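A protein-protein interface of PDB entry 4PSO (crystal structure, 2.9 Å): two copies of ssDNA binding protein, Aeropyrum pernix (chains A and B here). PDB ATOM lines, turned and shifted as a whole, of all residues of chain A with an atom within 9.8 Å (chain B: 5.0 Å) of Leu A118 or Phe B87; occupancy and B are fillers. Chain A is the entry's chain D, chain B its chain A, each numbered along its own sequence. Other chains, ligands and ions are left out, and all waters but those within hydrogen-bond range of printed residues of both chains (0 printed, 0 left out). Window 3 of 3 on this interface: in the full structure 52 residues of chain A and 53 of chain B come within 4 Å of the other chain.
Val A107 touches Leu B90 (CG1 to O, 3.6 Å). Phe A110 touches Val B53. Phe B87 touches Ala A111 (O to CB, 3.2 Å). CB of Ala A114 touches CD1 of Phe B87, at 3.5 Å. CD1 of Leu A118 touches O of Asn B49 (3.4 Å). Leu A118 touches Leu B50. Leu A118 touches Val B53 (CD1 to CG2, 3.6 Å). CD1 of Leu A118 touches CZ of Phe B87, 3.9 Å away.
Leu A118 touches just these residues of chain B: Asn B49 (3.4 Å), Leu B50 (3.9 Å), Val B53 (3.6 Å) and Phe B87 (3.9 Å). Of the printed residues of chain A, Phe B87 touches Ala A111 (3.2 Å), Ala A114 (3.5 Å) and Leu A118 (3.9 Å). Asn B49 touches just one residue of chain A: Leu A118. No residue of chain A comes within 4 Å of Asp B86. Ser B88 touches none of the printed residues of chain A. No residue of chain A comes within 4 Å of Thr B89. Printed residues of chain B within 4 Å of Phe A110: Val B53. Of the printed residues of chain B, Ala A114 touches Phe B87 (3.5 Å). Of the printed residues of chain B, Ala A111 touches Phe B87. Printed residues of chain B within 4 Å of Val A107: Leu B90. Printed residues of chain A within 4 Å of Val B53: Phe A110 (3.2 Å) and Leu A118 (3.6 Å). The nearest residue of chain B that does not touch Leu A118 is Phe B85 (4.9 Å).
Printed residues of chain A that touch a printed residue of chain B: Val A107, Phe A110, Ala A111, Ala A114 and Leu A118. Hydrophobic or aromatic side chains of chain A within 4 Å of the printed part of chain B: Val A107, Phe A110, Ala A111, Ala A114 and Leu A118. Hydrophobic or aromatic side chains of chain B that line the printed part of chain A: Val B53, Phe B87 and Leu B90. Among the printed residues, 8 pairs touch across the chains. Among the printed residues, no Asp or Glu carboxylate lies within 4 Å of a Lys or Arg side-chain nitrogen of the other chain.
No position is printed for both chains.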
ATOM      1  N   ALA A 104      19.991 -21.644 -17.128  1.00  0.00           N
ATOM      2  CA  ALA A 104      20.748 -22.192 -16.002  1.00  0.00           C
ATOM      3  C   ALA A 104      21.462 -21.124 -15.158  1.00  0.00           C
ATOM      4  O   ALA A 104      21.405 -21.183 -13.929  1.00  0.00           O
ATOM      5  CB  ALA A 104      21.750 -23.234 -16.497  1.00  0.00           C
ATOM      6  N   ILE A 106      20.634 -17.982 -14.830  1.00  0.00           N
ATOM      7  CA  ILE A 106      19.603 -17.161 -14.199  1.00  0.00           C
ATOM      8  C   ILE A 106      18.966 -17.874 -13.007  1.00  0.00           C
ATOM      9  O   ILE A 106      18.731 -17.266 -11.960  1.00  0.00           O
ATOM     10  CB  ILE A 106      18.492 -16.770 -15.199  1.00  0.00           C
ATOM     11  CG1 ILE A 106      19.070 -15.989 -16.385  1.00  0.00           C
ATOM     12  CG2 ILE A 106      17.421 -15.951 -14.504  1.00  0.00           C
ATOM     13  CD1 ILE A 106      18.017 -15.528 -17.386  1.00  0.00           C
ATOM     14  N   VAL A 107      18.700 -19.168 -13.168  1.00  0.00           N
ATOM     15  CA  VAL A 107      18.127 -19.977 -12.096  1.00  0.00           C
ATOM     16  C   VAL A 107      19.126 -20.124 -10.949  1.00  0.00           C
ATOM     17  O   VAL A 107      18.756 -20.046  -9.777  1.00  0.00           O
ATOM     18  CB  VAL A 107      17.704 -21.370 -12.609  1.00  0.00           C
ATOM     19  CG1 VAL A 107      17.272 -22.272 -11.459  1.00  0.00           C
ATOM     20  CG2 VAL A 107      16.586 -21.233 -13.628  1.00  0.00           C
ATOM     21  N   GLU A 108      20.391 -20.339 -11.302  1.00  0.00           N
ATOM     22  CA  GLU A 108      21.459 -20.493 -10.321  1.00  0.00           C
ATOM     23  C   GLU A 108      21.634 -19.210  -9.513  1.00  0.00           C
ATOM     24  O   GLU A 108      21.852 -19.255  -8.301  1.00  0.00           O
ATOM     25  CB  GLU A 108      22.773 -20.879 -11.004  1.00  0.00           C
ATOM     26  CG  GLU A 108      23.896 -21.204 -10.033  1.00  0.00           C
ATOM     27  CD  GLU A 108      25.192 -21.561 -10.734  1.00  0.00           C
ATOM     28  OE1 GLU A 108      25.273 -21.381 -11.967  1.00  0.00           O
ATOM     29  OE2 GLU A 108      26.131 -22.024 -10.051  1.00  0.00           O
ATOM     30  N   ASP A 109      21.539 -18.071 -10.198  1.00  0.00           N
ATOM     31  CA  ASP A 109      21.685 -16.767  -9.564  1.00  0.00           C
ATOM     32  C   ASP A 109      20.541 -16.566  -8.584  1.00  0.00           C
ATOM     33  O   ASP A 109      20.731 -16.092  -7.465  1.00  0.00           O
ATOM     34  CB  ASP A 109      21.642 -15.641 -10.603  1.00  0.00           C
ATOM     35  CG  ASP A 109      22.967 -15.421 -11.306  1.00  0.00           C
ATOM     36  OD1 ASP A 109      23.996 -15.969 -10.860  1.00  0.00           O
ATOM     37  OD2 ASP A 109      22.967 -14.692 -12.322  1.00  0.00           O
ATOM     38  N   PHE A 110      19.349 -16.936  -9.034  1.00  0.00           N
ATOM     39  CA  PHE A 110      18.129 -16.795  -8.256  1.00  0.00           C
ATOM     40  C   PHE A 110      18.118 -17.755  -7.067  1.00  0.00           C
ATOM     41  O   PHE A 110      17.556 -17.456  -6.014  1.00  0.00           O
ATOM     42  CB  PHE A 110      16.918 -17.033  -9.159  1.00  0.00           C
ATOM     43  CG  PHE A 110      15.604 -16.713  -8.518  1.00  0.00           C
ATOM     44  CD1 PHE A 110      14.887 -17.685  -7.841  1.00  0.00           C
ATOM     45  CD2 PHE A 110      15.074 -15.436  -8.612  1.00  0.00           C
ATOM     46  CE1 PHE A 110      13.669 -17.385  -7.260  1.00  0.00           C
ATOM     47  CE2 PHE A 110      13.857 -15.129  -8.033  1.00  0.00           C
ATOM     48  CZ  PHE A 110      13.154 -16.106  -7.355  1.00  0.00           C
ATOM     49  N   ALA A 111      18.732 -18.918  -7.255  1.00  0.00           N
ATOM     50  CA  ALA A 111      18.760 -19.957  -6.233  1.00  0.00           C
ATOM     51  C   ALA A 111      19.535 -19.522  -4.993  1.00  0.00           C
ATOM     52  O   ALA A 111      19.321 -20.050  -3.902  1.00  0.00           O
ATOM     53  CB  ALA A 111      19.360 -21.229  -6.798  1.00  0.00           C
ATOM     54  N   ARG A 112      20.445 -18.570  -5.168  1.00  0.00           N
ATOM     55  CA  ARG A 112      21.243 -18.077  -4.054  1.00  0.00           C
ATOM     56  C   ARG A 112      20.425 -17.123  -3.184  1.00  0.00           C
ATOM     57  O   ARG A 112      20.645 -17.028  -1.976  1.00  0.00           O
ATOM     58  CB  ARG A 112      22.516 -17.388  -4.565  1.00  0.00           C
ATOM     59  CG  ARG A 112      23.475 -18.327  -5.300  1.00  0.00           C
ATOM     60  CD  ARG A 112      24.815 -17.659  -5.610  1.00  0.00           C
ATOM     61  NE  ARG A 112      24.720 -16.578  -6.592  1.00  0.00           N
ATOM     62  CZ  ARG A 112      24.891 -16.738  -7.901  1.00  0.00           C
ATOM     63  NH1 ARG A 112      25.171 -17.937  -8.397  1.00  0.00           N
ATOM     64  NH2 ARG A 112      24.790 -15.697  -8.718  1.00  0.00           N
ATOM     65  N   ALA A 113      19.481 -16.422  -3.804  1.00  0.00           N
ATOM     66  CA  ALA A 113      18.660 -15.444  -3.096  1.00  0.00           C
ATOM     67  C   ALA A 113      17.343 -16.055  -2.622  1.00  0.00           C
ATOM     68  O   ALA A 113      16.575 -15.422  -1.899  1.00  0.00           O
ATOM     69  CB  ALA A 113      18.392 -14.247  -3.988  1.00  0.00           C
ATOM     70  N   ALA A 114      17.094 -17.289  -3.045  1.00  0.00           N
ATOM     71  CA  ALA A 114      15.832 -17.976  -2.774  1.00  0.00           C
ATOM     72  C   ALA A 114      15.526 -18.258  -1.291  1.00  0.00           C
ATOM     73  O   ALA A 114      14.384 -18.073  -0.865  1.00  0.00           O
ATOM     74  CB  ALA A 114      15.779 -19.276  -3.564  1.00  0.00           C
ATOM     75  N   PRO A 115      16.520 -18.725  -0.503  1.00  0.00           N
ATOM     76  CA  PRO A 115      16.171 -19.018   0.896  1.00  0.00           C
ATOM     77  C   PRO A 115      15.764 -17.791   1.712  1.00  0.00           C
ATOM     78  O   PRO A 115      15.058 -17.942   2.711  1.00  0.00           O
ATOM     79  CB  PRO A 115      17.460 -19.634   1.455  1.00  0.00           C
ATOM     80  CG  PRO A 115      18.169 -20.174   0.263  1.00  0.00           C
ATOM     81  CD  PRO A 115      17.885 -19.187  -0.823  1.00  0.00           C
ATOM     82  N   ARG A 116      16.198 -16.603   1.300  1.00  0.00           N
ATOM     83  CA  ARG A 116      15.764 -15.372   1.956  1.00  0.00           C
ATOM     84  C   ARG A 116      14.315 -15.054   1.625  1.00  0.00           C
ATOM     85  O   ARG A 116      13.527 -14.688   2.498  1.00  0.00           O
ATOM     86  CB  ARG A 116      16.640 -14.188   1.543  1.00  0.00           C
ATOM     87  CG  ARG A 116      16.180 -12.866   2.148  1.00  0.00           C
ATOM     88  CD  ARG A 116      17.056 -11.696   1.734  1.00  0.00           C
ATOM     89  NE  ARG A 116      18.451 -11.881   2.118  1.00  0.00           N
ATOM     90  CZ  ARG A 116      19.414 -10.998   1.871  1.00  0.00           C
ATOM     91  NH1 ARG A 116      20.658 -11.241   2.258  1.00  0.00           N
ATOM     92  NH2 ARG A 116      19.131  -9.872   1.233  1.00  0.00           N
ATOM     93  N   LEU A 117      13.984 -15.188   0.346  1.00  0.00           N
ATOM     94  CA  LEU A 117      12.648 -14.898  -0.154  1.00  0.00           C
ATOM     95  C   LEU A 117      11.621 -15.883   0.391  1.00  0.00           C
ATOM     96  O   LEU A 117      10.444 -15.550   0.530  1.00  0.00           O
ATOM     97  CB  LEU A 117      12.649 -14.928  -1.682  1.00  0.00           C
ATOM     98  CG  LEU A 117      13.654 -13.971  -2.329  1.00  0.00           C
ATOM     99  CD1 LEU A 117      13.548 -13.994  -3.848  1.00  0.00           C
ATOM    100  CD2 LEU A 117      13.486 -12.559  -1.786  1.00  0.00           C
ATOM    101  N   LEU A 118      12.078 -17.096   0.693  1.00  0.00           N
ATOM    102  CA  LEU A 118      11.189 -18.170   1.118  1.00  0.00           C
ATOM    103  C   LEU A 118      10.532 -17.893   2.467  1.00  0.00           C
ATOM    104  O   LEU A 118       9.424 -18.362   2.728  1.00  0.00           O
ATOM    105  CB  LEU A 118      11.978 -19.481   1.202  1.00  0.00           C
ATOM    106  CG  LEU A 118      11.262 -20.830   1.311  1.00  0.00           C
ATOM    107  CD1 LEU A 118      10.630 -21.217  -0.008  1.00  0.00           C
ATOM    108  CD2 LEU A 118      12.224 -21.913   1.788  1.00  0.00           C
ATOM    109  N   GLU A 119      11.208 -17.127   3.320  1.00  0.00           N
ATOM    110  CA  GLU A 119      10.668 -16.828   4.642  1.00  0.00           C
ATOM    111  C   GLU A 119       9.939 -15.489   4.680  1.00  0.00           C
ATOM    112  O   GLU A 119       9.003 -15.318   5.464  1.00  0.00           O
ATOM    113  CB  GLU A 119      11.766 -16.844   5.710  1.00  0.00           C
ATOM    114  CG  GLU A 119      11.224 -16.582   7.119  1.00  0.00           C
ATOM    115  CD  GLU A 119      12.303 -16.486   8.175  1.00  0.00           C
ATOM    116  OE1 GLU A 119      13.491 -16.635   7.828  1.00  0.00           O
ATOM    117  OE2 GLU A 119      11.959 -16.261   9.356  1.00  0.00           O
ATOM    118  N   GLU A 120      10.357 -14.544   3.837  1.00  0.00           N
ATOM    119  CA  GLU A 120       9.771 -13.208   3.896  1.00  0.00           C
ATOM    120  C   GLU A 120       8.276 -13.246   3.652  1.00  0.00           C
ATOM    121  O   GLU A 120       7.780 -13.988   2.804  1.00  0.00           O
ATOM    122  CB  GLU A 120      10.411 -12.247   2.884  1.00  0.00           C
ATOM    123  CG  GLU A 120      11.791 -11.725   3.250  1.00  0.00           C
ATOM    124  CD  GLU A 120      12.335 -10.764   2.206  1.00  0.00           C
ATOM    125  OE1 GLU A 120      11.660 -10.558   1.174  1.00  0.00           O
ATOM    126  OE2 GLU A 120      13.429 -10.200   2.424  1.00  0.00           O
ATOM    127  N   GLU A 121       7.572 -12.421   4.412  1.00  0.00           N
ATOM    128  CA  GLU A 121       6.143 -12.260   4.259  1.00  0.00           C
ATOM    129  C   GLU A 121       5.973 -11.382   3.019  1.00  0.00           C
ATOM    130  O   GLU A 121       6.808 -10.516   2.743  1.00  0.00           O
ATOM    131  CB  GLU A 121       5.535 -11.679   5.537  1.00  0.00           C
ATOM    132  CG  GLU A 121       4.086 -11.257   5.480  1.00  0.00           C
ATOM    133  CD  GLU A 121       3.614 -10.771   6.838  1.00  0.00           C
ATOM    134  OE1 GLU A 121       4.270 -11.112   7.847  1.00  0.00           O
ATOM    135  OE2 GLU A 121       2.599 -10.053   6.908  1.00  0.00           O
ATOM    136  N   ILE A 122       4.896 -11.607   2.278  1.00  0.00           N
ATOM    137  CA  ILE A 122       4.759 -11.079   0.921  1.00  0.00           C
ATOM    138  C   ILE A 122       4.448  -9.586   0.764  1.00  0.00           C
ATOM    139  O   ILE A 122       4.903  -8.960  -0.202  1.00  0.00           O
ATOM    140  CB  ILE A 122       3.655 -11.879   0.188  1.00  0.00           C
ATOM    141  CG1 ILE A 122       3.898 -13.380   0.355  1.00  0.00           C
ATOM    142  CG2 ILE A 122       3.618 -11.549  -1.281  1.00  0.00           C
ATOM    143  CD1 ILE A 122       2.864 -14.249  -0.335  1.00  0.00           C
ATOM    144  N   THR A 170       1.384 -16.663  -4.646  1.00  0.00           N
ATOM    145  CA  THR A 170       0.992 -18.033  -4.332  1.00  0.00           C
ATOM    146  C   THR A 170      -0.459 -18.035  -3.864  1.00  0.00           C
ATOM    147  O   THR A 170      -0.887 -17.113  -3.171  1.00  0.00           O
ATOM    148  CB  THR A 170       1.907 -18.666  -3.258  1.00  0.00           C
ATOM    149  OG1 THR A 170       1.514 -20.027  -3.030  1.00  0.00           O
ATOM    150  CG2 THR A 170       1.825 -17.892  -1.949  1.00  0.00           C
ATOM    151  N   ASN A 203      -2.578 -21.983   2.529  1.00  0.00           N
ATOM    152  CA  ASN A 203      -2.036 -22.301   1.220  1.00  0.00           C
ATOM    153  C   ASN A 203      -2.957 -23.297   0.535  1.00  0.00           C
ATOM    154  O   ASN A 203      -3.087 -24.440   0.979  1.00  0.00           O
ATOM    155  CB  ASN A 203      -0.620 -22.855   1.340  1.00  0.00           C
ATOM    156  CG  ASN A 203       0.341 -21.851   1.935  1.00  0.00           C
ATOM    157  OD1 ASN A 203       0.583 -21.840   3.142  1.00  0.00           O
ATOM    158  ND2 ASN A 203       0.889 -20.988   1.087  1.00  0.00           N
ATOM    159  N   ASN B  49       5.314 -21.820  -0.224  1.00  0.00           N
ATOM    160  CA  ASN B  49       6.523 -21.009  -0.170  1.00  0.00           C
ATOM    161  C   ASN B  49       7.399 -21.223  -1.402  1.00  0.00           C
ATOM    162  O   ASN B  49       8.011 -20.280  -1.903  1.00  0.00           O
ATOM    163  CB  ASN B  49       7.316 -21.308   1.104  1.00  0.00           C
ATOM    164  CG  ASN B  49       6.671 -20.721   2.348  1.00  0.00           C
ATOM    165  OD1 ASN B  49       5.961 -19.716   2.281  1.00  0.00           O
ATOM    166  ND2 ASN B  49       6.921 -21.345   3.493  1.00  0.00           N
ATOM    167  N   LEU B  50       7.453 -22.460  -1.892  1.00  0.00           N
ATOM    168  CA  LEU B  50       8.208 -22.768  -3.105  1.00  0.00           C
ATOM    169  C   LEU B  50       7.578 -22.080  -4.315  1.00  0.00           C
ATOM    170  O   LEU B  50       8.281 -21.512  -5.151  1.00  0.00           O
ATOM    171  CB  LEU B  50       8.283 -24.280  -3.334  1.00  0.00           C
ATOM    172  CG  LEU B  50       9.028 -24.745  -4.595  1.00  0.00           C
ATOM    173  CD1 LEU B  50      10.479 -24.283  -4.579  1.00  0.00           C
ATOM    174  CD2 LEU B  50       8.952 -26.257  -4.766  1.00  0.00           C
ATOM    175  N   VAL B  53       8.395 -18.521  -4.459  1.00  0.00           N
ATOM    176  CA  VAL B  53       9.745 -18.362  -4.980  1.00  0.00           C
ATOM    177  C   VAL B  53       9.785 -18.506  -6.498  1.00  0.00           C
ATOM    178  O   VAL B  53      10.404 -17.702  -7.193  1.00  0.00           O
ATOM    179  CB  VAL B  53      10.698 -19.394  -4.342  1.00  0.00           C
ATOM    180  CG1 VAL B  53      12.020 -19.454  -5.087  1.00  0.00           C
ATOM    181  CG2 VAL B  53      10.913 -19.073  -2.869  1.00  0.00           C
ATOM    182  N   ILE B  74      13.344 -30.058  -8.085  1.00  0.00           N
ATOM    183  CA  ILE B  74      14.162 -29.628  -6.961  1.00  0.00           C
ATOM    184  C   ILE B  74      14.187 -30.709  -5.885  1.00  0.00           C
ATOM    185  O   ILE B  74      13.168 -31.343  -5.602  1.00  0.00           O
ATOM    186  CB  ILE B  74      13.648 -28.284  -6.367  1.00  0.00           C
ATOM    187  CG1 ILE B  74      14.546 -27.826  -5.213  1.00  0.00           C
ATOM    188  CG2 ILE B  74      12.197 -28.403  -5.903  1.00  0.00           C
ATOM    189  CD1 ILE B  74      14.173 -26.477  -4.640  1.00  0.00           C
ATOM    190  N   PHE B  85      14.013 -27.362   1.288  1.00  0.00           N
ATOM    191  CA  PHE B  85      14.463 -27.479  -0.095  1.00  0.00           C
ATOM    192  C   PHE B  85      15.944 -27.165  -0.281  1.00  0.00           C
ATOM    193  O   PHE B  85      16.493 -26.277   0.371  1.00  0.00           O
ATOM    194  CB  PHE B  85      13.626 -26.571  -1.002  1.00  0.00           C
ATOM    195  CG  PHE B  85      12.171 -26.950  -1.067  1.00  0.00           C
ATOM    196  CD1 PHE B  85      11.754 -27.994  -1.885  1.00  0.00           C
ATOM    197  CD2 PHE B  85      11.220 -26.265  -0.322  1.00  0.00           C
ATOM    198  CE1 PHE B  85      10.418 -28.354  -1.953  1.00  0.00           C
ATOM    199  CE2 PHE B  85       9.880 -26.619  -0.386  1.00  0.00           C
ATOM    200  CZ  PHE B  85       9.480 -27.665  -1.205  1.00  0.00           C
ATOM    201  N   ASP B  86      16.575 -27.910  -1.183  1.00  0.00           N
ATOM    202  CA  ASP B  86      17.955 -27.670  -1.579  1.00  0.00           C
ATOM    203  C   ASP B  86      17.945 -26.916  -2.902  1.00  0.00           C
ATOM    204  O   ASP B  86      17.816 -27.520  -3.967  1.00  0.00           O
ATOM    205  CB  ASP B  86      18.711 -28.995  -1.707  1.00  0.00           C
ATOM    206  CG  ASP B  86      20.213 -28.815  -1.810  1.00  0.00           C
ATOM    207  OD1 ASP B  86      20.673 -27.705  -2.156  1.00  0.00           O
ATOM    208  OD2 ASP B  86      20.937 -29.802  -1.551  1.00  0.00           O
ATOM    209  N   PHE B  87      18.067 -25.594  -2.829  1.00  0.00           N
ATOM    210  CA  PHE B  87      17.912 -24.749  -4.008  1.00  0.00           C
ATOM    211  C   PHE B  87      19.093 -24.847  -4.970  1.00  0.00           C
ATOM    212  O   PHE B  87      19.046 -24.306  -6.073  1.00  0.00           O
ATOM    213  CB  PHE B  87      17.694 -23.296  -3.583  1.00  0.00           C
ATOM    214  CG  PHE B  87      16.338 -23.043  -2.989  1.00  0.00           C
ATOM    215  CD1 PHE B  87      15.249 -22.775  -3.806  1.00  0.00           C
ATOM    216  CD2 PHE B  87      16.145 -23.091  -1.616  1.00  0.00           C
ATOM    217  CE1 PHE B  87      13.993 -22.547  -3.266  1.00  0.00           C
ATOM    218  CE2 PHE B  87      14.891 -22.864  -1.067  1.00  0.00           C
ATOM    219  CZ  PHE B  87      13.814 -22.591  -1.895  1.00  0.00           C
ATOM    220  N   SER B  88      20.145 -25.546  -4.555  1.00  0.00           N
ATOM    221  CA  SER B  88      21.274 -25.811  -5.437  1.00  0.00           C
ATOM    222  C   SER B  88      20.883 -26.844  -6.489  1.00  0.00           C
ATOM    223  O   SER B  88      21.538 -26.968  -7.527  1.00  0.00           O
ATOM    224  CB  SER B  88      22.482 -26.298  -4.636  1.00  0.00           C
ATOM    225  OG  SER B  88      22.180 -27.484  -3.920  1.00  0.00           O
ATOM    226  N   THR B  89      19.806 -27.578  -6.214  1.00  0.00           N
ATOM    227  CA  THR B  89      19.329 -28.619  -7.119  1.00  0.00           C
ATOM    228  C   THR B  89      18.159 -28.134  -7.971  1.00  0.00           C
ATOM    229  O   THR B  89      17.620 -28.896  -8.772  1.00  0.00           O
ATOM    230  CB  THR B  89      18.885 -29.886  -6.358  1.00  0.00           C
ATOM    231  OG1 THR B  89      17.751 -29.582  -5.533  1.00  0.00           O
ATOM    232  CG2 THR B  89      20.020 -30.431  -5.499  1.00  0.00           C
ATOM    233  N   LEU B  90      17.761 -26.875  -7.793  1.00  0.00           N
ATOM    234  CA  LEU B  90      16.648 -26.324  -8.562  1.00  0.00           C
ATOM    235  C   LEU B  90      16.984 -26.271 -10.043  1.00  0.00           C
ATOM    236  O   LEU B  90      17.998 -25.697 -10.442  1.00  0.00           O
ATOM    237  CB  LEU B  90      16.271 -24.923  -8.070  1.00  0.00           C
ATOM    238  CG  LEU B  90      15.173 -24.228  -8.887  1.00  0.00           C
ATOM    239  CD1 LEU B  90      13.855 -24.981  -8.774  1.00  0.00           C
ATOM    240  CD2 LEU B  90      14.997 -22.781  -8.458  1.00  0.00           C
